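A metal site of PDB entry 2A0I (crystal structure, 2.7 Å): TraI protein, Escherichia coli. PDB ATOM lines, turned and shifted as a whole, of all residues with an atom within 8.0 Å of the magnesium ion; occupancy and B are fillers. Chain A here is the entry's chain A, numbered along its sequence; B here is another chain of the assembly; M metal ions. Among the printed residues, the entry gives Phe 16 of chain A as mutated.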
ATOM      1  N   PHE A  16      12.035 -19.902  -9.569  1.00  0.00           N
ATOM      2  CA  PHE A  16      11.778 -19.502  -8.193  1.00  0.00           C
ATOM      3  C   PHE A  16      12.413 -20.434  -7.150  1.00  0.00           C
ATOM      4  O   PHE A  16      13.296 -20.016  -6.400  1.00  0.00           O
ATOM      5  CB  PHE A  16      10.264 -19.392  -7.996  1.00  0.00           C
ATOM      6  CG  PHE A  16       9.861 -18.818  -6.674  1.00  0.00           C
ATOM      7  CD1 PHE A  16       9.721 -19.639  -5.566  1.00  0.00           C
ATOM      8  CD2 PHE A  16       9.598 -17.461  -6.543  1.00  0.00           C
ATOM      9  CE1 PHE A  16       9.327 -19.109  -4.339  1.00  0.00           C
ATOM     10  CE2 PHE A  16       9.203 -16.927  -5.329  1.00  0.00           C
ATOM     11  CZ  PHE A  16       9.065 -17.757  -4.225  1.00  0.00           C
ATOM     12  N   TYR A  17      12.001 -21.701  -7.135  1.00  0.00           N
ATOM     13  CA  TYR A  17      12.516 -22.668  -6.172  1.00  0.00           C
ATOM     14  C   TYR A  17      13.967 -23.105  -6.398  1.00  0.00           C
ATOM     15  O   TYR A  17      14.655 -23.512  -5.460  1.00  0.00           O
ATOM     16  CB  TYR A  17      11.621 -23.905  -6.138  1.00  0.00           C
ATOM     17  CG  TYR A  17      10.167 -23.575  -5.906  1.00  0.00           C
ATOM     18  CD1 TYR A  17       9.326 -23.289  -6.974  1.00  0.00           C
ATOM     19  CD2 TYR A  17       9.633 -23.537  -4.622  1.00  0.00           C
ATOM     20  CE1 TYR A  17       7.992 -22.962  -6.777  1.00  0.00           C
ATOM     21  CE2 TYR A  17       8.287 -23.216  -4.410  1.00  0.00           C
ATOM     22  CZ  TYR A  17       7.481 -22.931  -5.490  1.00  0.00           C
ATOM     23  OH  TYR A  17       6.151 -22.624  -5.299  1.00  0.00           O
ATOM     24  N   ASP A  19      16.366 -21.353  -6.817  1.00  0.00           N
ATOM     25  CA  ASP A  19      17.276 -20.389  -6.185  1.00  0.00           C
ATOM     26  C   ASP A  19      17.282 -20.554  -4.666  1.00  0.00           C
ATOM     27  O   ASP A  19      16.376 -20.093  -3.977  1.00  0.00           O
ATOM     28  CB  ASP A  19      16.869 -18.957  -6.544  1.00  0.00           C
ATOM     29  CG  ASP A  19      17.064 -18.649  -8.019  1.00  0.00           C
ATOM     30  OD1 ASP A  19      18.194 -18.881  -8.524  1.00  0.00           O
ATOM     31  OD2 ASP A  19      16.095 -18.184  -8.661  1.00  0.00           O
ATOM     32  N   ASP A  81       1.934 -26.363  -3.936  1.00  0.00           N
ATOM     33  CA  ASP A  81       3.004 -26.063  -2.987  1.00  0.00           C
ATOM     34  C   ASP A  81       2.432 -26.186  -1.568  1.00  0.00           C
ATOM     35  O   ASP A  81       1.462 -25.492  -1.227  1.00  0.00           O
ATOM     36  CB  ASP A  81       3.530 -24.641  -3.212  1.00  0.00           C
ATOM     37  CG  ASP A  81       4.790 -24.322  -2.409  1.00  0.00           C
ATOM     38  OD1 ASP A  81       5.087 -25.034  -1.417  1.00  0.00           O
ATOM     39  OD2 ASP A  81       5.497 -23.350  -2.767  1.00  0.00           O
ATOM     40  N   THR A  83       3.659 -25.612   1.996  1.00  0.00           N
ATOM     41  CA  THR A  83       4.780 -25.065   2.745  1.00  0.00           C
ATOM     42  C   THR A  83       4.648 -25.232   4.241  1.00  0.00           C
ATOM     43  O   THR A  83       3.719 -24.741   4.852  1.00  0.00           O
ATOM     44  CB  THR A  83       4.943 -23.605   2.427  1.00  0.00           C
ATOM     45  OG1 THR A  83       5.167 -23.451   1.022  1.00  0.00           O
ATOM     46  CG2 THR A  83       6.118 -23.028   3.209  1.00  0.00           C
ATOM     47  N   SER A  85       5.990 -24.248   7.690  1.00  0.00           N
ATOM     48  CA  SER A  85       6.818 -23.251   8.347  1.00  0.00           C
ATOM     49  C   SER A  85       7.059 -23.649   9.805  1.00  0.00           C
ATOM     50  O   SER A  85       6.113 -23.996  10.531  1.00  0.00           O
ATOM     51  CB  SER A  85       6.164 -21.889   8.274  1.00  0.00           C
ATOM     52  OG  SER A  85       6.020 -21.523   6.930  1.00  0.00           O
ATOM     53  N   PHE A 144      12.037 -27.835  -1.267  1.00  0.00           N
ATOM     54  CA  PHE A 144      13.032 -26.769  -1.176  1.00  0.00           C
ATOM     55  C   PHE A 144      13.012 -26.187   0.236  1.00  0.00           C
ATOM     56  O   PHE A 144      11.957 -25.990   0.819  1.00  0.00           O
ATOM     57  CB  PHE A 144      12.734 -25.705  -2.214  1.00  0.00           C
ATOM     58  CG  PHE A 144      12.282 -26.268  -3.530  1.00  0.00           C
ATOM     59  CD1 PHE A 144      10.967 -26.667  -3.715  1.00  0.00           C
ATOM     60  CD2 PHE A 144      13.187 -26.433  -4.570  1.00  0.00           C
ATOM     61  CE1 PHE A 144      10.551 -27.238  -4.918  1.00  0.00           C
ATOM     62  CE2 PHE A 144      12.784 -26.998  -5.787  1.00  0.00           C
ATOM     63  CZ  PHE A 144      11.454 -27.393  -5.955  1.00  0.00           C
ATOM     64  N   ASN A 145      14.203 -25.918   0.788  1.00  0.00           N
ATOM     65  CA  ASN A 145      14.311 -25.357   2.122  1.00  0.00           C
ATOM     66  C   ASN A 145      14.825 -23.926   2.101  1.00  0.00           C
ATOM     67  O   ASN A 145      15.770 -23.614   1.387  1.00  0.00           O
ATOM     68  CB  ASN A 145      15.268 -26.207   2.979  1.00  0.00           C
ATOM     69  CG  ASN A 145      14.634 -27.483   3.509  1.00  0.00           C
ATOM     70  OD1 ASN A 145      15.260 -28.237   4.241  1.00  0.00           O
ATOM     71  ND2 ASN A 145      13.381 -27.709   3.131  1.00  0.00           N
ATOM     72  N   HIS A 146      14.187 -23.053   2.882  1.00  0.00           N
ATOM     73  CA  HIS A 146      14.591 -21.654   2.988  1.00  0.00           C
ATOM     74  C   HIS A 146      14.641 -21.297   4.476  1.00  0.00           C
ATOM     75  O   HIS A 146      14.109 -22.046   5.296  1.00  0.00           O
ATOM     76  CB  HIS A 146      13.579 -20.759   2.297  1.00  0.00           C
ATOM     77  CG  HIS A 146      13.270 -21.168   0.893  1.00  0.00           C
ATOM     78  ND1 HIS A 146      12.203 -20.655   0.186  1.00  0.00           N
ATOM     79  CD2 HIS A 146      13.883 -22.040   0.063  1.00  0.00           C
ATOM     80  CE1 HIS A 146      12.171 -21.202  -1.019  1.00  0.00           C
ATOM     81  NE2 HIS A 146      13.184 -22.047  -1.120  1.00  0.00           N
ATOM     82  N   ASP A 147      15.253 -20.176   4.829  1.00  0.00           N
ATOM     83  CA  ASP A 147      15.324 -19.804   6.245  1.00  0.00           C
ATOM     84  C   ASP A 147      15.008 -18.352   6.593  1.00  0.00           C
ATOM     85  O   ASP A 147      15.308 -17.895   7.701  1.00  0.00           O
ATOM     86  CB  ASP A 147      16.704 -20.162   6.833  1.00  0.00           C
ATOM     87  CG  ASP A 147      17.866 -19.634   5.998  1.00  0.00           C
ATOM     88  OD1 ASP A 147      17.708 -18.623   5.271  1.00  0.00           O
ATOM     89  OD2 ASP A 147      18.964 -20.231   6.093  1.00  0.00           O
ATOM     90  N   THR A 148      14.409 -17.610   5.669  1.00  0.00           N
ATOM     91  CA  THR A 148      14.081 -16.231   5.975  1.00  0.00           C
ATOM     92  C   THR A 148      12.661 -15.873   5.576  1.00  0.00           C
ATOM     93  O   THR A 148      11.974 -16.640   4.890  1.00  0.00           O
ATOM     94  CB  THR A 148      15.054 -15.242   5.270  1.00  0.00           C
ATOM     95  OG1 THR A 148      14.945 -15.386   3.849  1.00  0.00           O
ATOM     96  CG2 THR A 148      16.481 -15.509   5.687  1.00  0.00           C
ATOM     97  N   SER A 149      12.213 -14.719   6.043  1.00  0.00           N
ATOM     98  CA  SER A 149      10.889 -14.222   5.719  1.00  0.00           C
ATOM     99  C   SER A 149      11.198 -13.127   4.726  1.00  0.00           C
ATOM    100  O   SER A 149      12.357 -12.760   4.561  1.00  0.00           O
ATOM    101  CB  SER A 149      10.204 -13.657   6.971  1.00  0.00           C
ATOM    102  OG  SER A 149      10.904 -12.562   7.558  1.00  0.00           O
ATOM    103  N   ARG A 150      10.182 -12.606   4.053  1.00  0.00           N
ATOM    104  CA  ARG A 150      10.424 -11.529   3.091  1.00  0.00           C
ATOM    105  C   ARG A 150      10.874 -10.292   3.855  1.00  0.00           C
ATOM    106  O   ARG A 150      11.362  -9.327   3.272  1.00  0.00           O
ATOM    107  CB  ARG A 150       9.173 -11.248   2.261  1.00  0.00           C
ATOM    108  CG  ARG A 150       8.780 -12.405   1.329  1.00  0.00           C
ATOM    109  CD  ARG A 150       9.882 -12.718   0.316  1.00  0.00           C
ATOM    110  NE  ARG A 150       9.493 -12.350  -1.047  1.00  0.00           N
ATOM    111  CZ  ARG A 150       8.567 -12.976  -1.757  1.00  0.00           C
ATOM    112  NH1 ARG A 150       7.922 -14.021  -1.264  1.00  0.00           N
ATOM    113  NH2 ARG A 150       8.276 -12.551  -2.981  1.00  0.00           N
ATOM    114  N   GLN A 155      13.174 -17.571   9.433  1.00  0.00           N
ATOM    115  CA  GLN A 155      11.877 -18.155   9.171  1.00  0.00           C
ATOM    116  C   GLN A 155      12.082 -19.389   8.328  1.00  0.00           C
ATOM    117  O   GLN A 155      11.769 -19.390   7.139  1.00  0.00           O
ATOM    118  CB  GLN A 155      10.981 -17.154   8.433  1.00  0.00           C
ATOM    119  CG  GLN A 155       9.580 -17.659   8.071  1.00  0.00           C
ATOM    120  CD  GLN A 155       8.791 -18.151   9.279  1.00  0.00           C
ATOM    121  OE1 GLN A 155       8.983 -17.691  10.391  1.00  0.00           O
ATOM    122  NE2 GLN A 155       7.883 -19.096   9.037  1.00  0.00           N
ATOM    123  N   LEU A 156      12.633 -20.418   8.959  1.00  0.00           N
ATOM    124  CA  LEU A 156      12.928 -21.699   8.316  1.00  0.00           C
ATOM    125  C   LEU A 156      11.666 -22.467   7.879  1.00  0.00           C
ATOM    126  O   LEU A 156      10.808 -22.791   8.706  1.00  0.00           O
ATOM    127  CB  LEU A 156      13.749 -22.560   9.287  1.00  0.00           C
ATOM    128  CG  LEU A 156      13.858 -24.062   9.071  1.00  0.00           C
ATOM    129  CD1 LEU A 156      14.693 -24.391   7.843  1.00  0.00           C
ATOM    130  CD2 LEU A 156      14.477 -24.652  10.303  1.00  0.00           C
ATOM    131  N   HIS A 157      11.560 -22.767   6.590  1.00  0.00           N
ATOM    132  CA  HIS A 157      10.408 -23.490   6.058  1.00  0.00           C
ATOM    133  C   HIS A 157      10.773 -24.329   4.826  1.00  0.00           C
ATOM    134  O   HIS A 157      11.806 -24.130   4.212  1.00  0.00           O
ATOM    135  CB  HIS A 157       9.299 -22.514   5.682  1.00  0.00           C
ATOM    136  CG  HIS A 157       9.720 -21.501   4.669  1.00  0.00           C
ATOM    137  ND1 HIS A 157      10.825 -20.693   4.830  1.00  0.00           N
ATOM    138  CD2 HIS A 157       9.154 -21.130   3.486  1.00  0.00           C
ATOM    139  CE1 HIS A 157      10.925 -19.870   3.801  1.00  0.00           C
ATOM    140  NE2 HIS A 157       9.924 -20.115   2.979  1.00  0.00           N
ATOM    141  N   THR A 158       9.886 -25.257   4.468  1.00  0.00           N
ATOM    142  CA  THR A 158      10.109 -26.122   3.323  1.00  0.00           C
ATOM    143  C   THR A 158       8.908 -26.096   2.385  1.00  0.00           C
ATOM    144  O   THR A 158       7.773 -26.305   2.807  1.00  0.00           O
ATOM    145  CB  THR A 158      10.334 -27.602   3.753  1.00  0.00           C
ATOM    146  OG1 THR A 158      11.477 -27.696   4.610  1.00  0.00           O
ATOM    147  CG2 THR A 158      10.551 -28.498   2.533  1.00  0.00           C
ATOM    148  N   HIS A 159       9.170 -25.823   1.122  1.00  0.00           N
ATOM    149  CA  HIS A 159       8.141 -25.820   0.101  1.00  0.00           C
ATOM    150  C   HIS A 159       8.116 -27.255  -0.400  1.00  0.00           C
ATOM    151  O   HIS A 159       9.052 -27.680  -1.089  1.00  0.00           O
ATOM    152  CB  HIS A 159       8.523 -24.925  -1.068  1.00  0.00           C
ATOM    153  CG  HIS A 159       8.431 -23.463  -0.784  1.00  0.00           C
ATOM    154  ND1 HIS A 159       7.239 -22.779  -0.756  1.00  0.00           N
ATOM    155  CD2 HIS A 159       9.396 -22.530  -0.580  1.00  0.00           C
ATOM    156  CE1 HIS A 159       7.473 -21.497  -0.557  1.00  0.00           C
ATOM    157  NE2 HIS A 159       8.777 -21.319  -0.450  1.00  0.00           N
ATOM    158  N   LYS A 265      11.288 -10.252  -3.029  1.00  0.00           N
ATOM    159  CA  LYS A 265      12.424 -11.101  -2.714  1.00  0.00           C
ATOM    160  C   LYS A 265      13.768 -10.398  -2.822  1.00  0.00           C
ATOM    161  O   LYS A 265      14.128  -9.859  -3.870  1.00  0.00           O
ATOM    162  CB  LYS A 265      12.394 -12.416  -3.506  1.00  0.00           C
ATOM    163  CG  LYS A 265      12.625 -13.582  -2.542  1.00  0.00           C
ATOM    164  CD  LYS A 265      12.409 -14.934  -3.163  1.00  0.00           C
ATOM    165  CE  LYS A 265      12.241 -15.983  -2.082  1.00  0.00           C
ATOM    166  NZ  LYS A 265      12.063 -17.339  -2.671  1.00  0.00           N
ATOM    167  P    DT B   8       6.263 -14.070   4.011  1.00  0.00           P
ATOM    168  OP1  DT B   8       7.675 -13.570   3.875  1.00  0.00           O
ATOM    169  OP2  DT B   8       5.209 -13.448   3.194  1.00  0.00           O
ATOM    170  O5'  DT B   8       6.324 -15.622   3.800  1.00  0.00           O
ATOM    171  C5'  DT B   8       7.533 -16.368   4.056  1.00  0.00           C
ATOM    172  C4'  DT B   8       7.485 -17.691   3.316  1.00  0.00           C
ATOM    173  O4'  DT B   8       6.236 -18.298   3.744  1.00  0.00           O
ATOM    174  C3'  DT B   8       7.377 -17.468   1.801  1.00  0.00           C
ATOM    175  O3'  DT B   8       8.323 -18.165   1.003  1.00  0.00           O
ATOM    176  C2'  DT B   8       5.982 -17.920   1.439  1.00  0.00           C
ATOM    177  C1'  DT B   8       5.346 -18.513   2.669  1.00  0.00           C
ATOM    178  N1   DT B   8       4.073 -17.778   2.941  1.00  0.00           N
ATOM    179  C2   DT B   8       3.204 -18.209   3.909  1.00  0.00           C
ATOM    180  O2   DT B   8       3.429 -19.148   4.642  1.00  0.00           O
ATOM    181  N3   DT B   8       2.044 -17.486   3.996  1.00  0.00           N
ATOM    182  C4   DT B   8       1.675 -16.386   3.219  1.00  0.00           C
ATOM    183  O4   DT B   8       0.587 -15.855   3.385  1.00  0.00           O
ATOM    184  C5   DT B   8       2.648 -15.972   2.252  1.00  0.00           C
ATOM    185  C7   DT B   8       2.376 -14.788   1.386  1.00  0.00           C
ATOM    186  C6   DT B   8       3.783 -16.677   2.165  1.00  0.00           C
ATOM    187  P    DG B   9       8.767 -17.507  -0.396  1.00  0.00           P
ATOM    188  OP1  DG B   9       9.862 -18.339  -0.953  1.00  0.00           O
ATOM    189  OP2  DG B   9       8.998 -16.064  -0.172  1.00  0.00           O
ATOM    190  O5'  DG B   9       7.490 -17.637  -1.342  1.00  0.00           O
ATOM    191  C5'  DG B   9       6.584 -18.725  -1.183  1.00  0.00           C
ATOM    192  C4'  DG B   9       5.759 -18.951  -2.431  1.00  0.00           C
ATOM    193  O4'  DG B   9       4.743 -19.912  -2.046  1.00  0.00           O
ATOM    194  C3'  DG B   9       5.004 -17.727  -2.933  1.00  0.00           C
ATOM    195  O3'  DG B   9       4.773 -17.824  -4.358  1.00  0.00           O
ATOM    196  C2'  DG B   9       3.693 -17.800  -2.174  1.00  0.00           C
ATOM    197  C1'  DG B   9       3.462 -19.301  -2.030  1.00  0.00           C
ATOM    198  N9   DG B   9       2.786 -19.682  -0.787  1.00  0.00           N
ATOM    199  C8   DG B   9       3.020 -20.792  -0.007  1.00  0.00           C
ATOM    200  N7   DG B   9       2.219 -20.872   1.018  1.00  0.00           N
ATOM    201  C5   DG B   9       1.429 -19.743   0.920  1.00  0.00           C
ATOM    202  C6   DG B   9       0.380 -19.282   1.749  1.00  0.00           C
ATOM    203  O6   DG B   9      -0.092 -19.806   2.760  1.00  0.00           O
ATOM    204  N1   DG B   9      -0.146 -18.082   1.297  1.00  0.00           N
ATOM    205  C2   DG B   9       0.281 -17.404   0.172  1.00  0.00           C
ATOM    206  N2   DG B   9      -0.343 -16.250  -0.105  1.00  0.00           N
ATOM    207  N3   DG B   9       1.241 -17.830  -0.608  1.00  0.00           N
ATOM    208  C4   DG B   9       1.768 -19.000  -0.186  1.00  0.00           C
HETATM  209 MG    MG M   1      10.267 -19.746   0.538  1.00  0.00          MG
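OP1 of DG 9 of chain B sits close to the side-chain amino group (NZ) of Lys 265 (3.0 Å).
The guanidinium group (NH1) of Arg 150 is in salt-bridge range of OP2 of DG 9 of chain B, 2.6 Å away.
ND1 of His 159 sits at hydrogen-bond distance from OG1 of Thr 83.
O of Phe 144 sits at hydrogen-bond distance from N of His 159.
OD2 of Asp 81 sits at hydrogen-bond distance from ND1 of His 159, 2.7 Å away.
ND1 of His 157 lies within hydrogen-bond range of O of Gln 155 (2.8 Å).
OP1 of DT 8 of chain B sits at hydrogen-bond distance from the backbone NH (N) of Arg 150.
Of the 21 residues printed, 5 come within 4 Å of the magnesium ion.
The magnesium ion is bound by OP1 of DG 9 of chain B, ND1 of His 146, NE2 of His 159, NE2 of His 157 and O3' of DT 8 of chain B.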
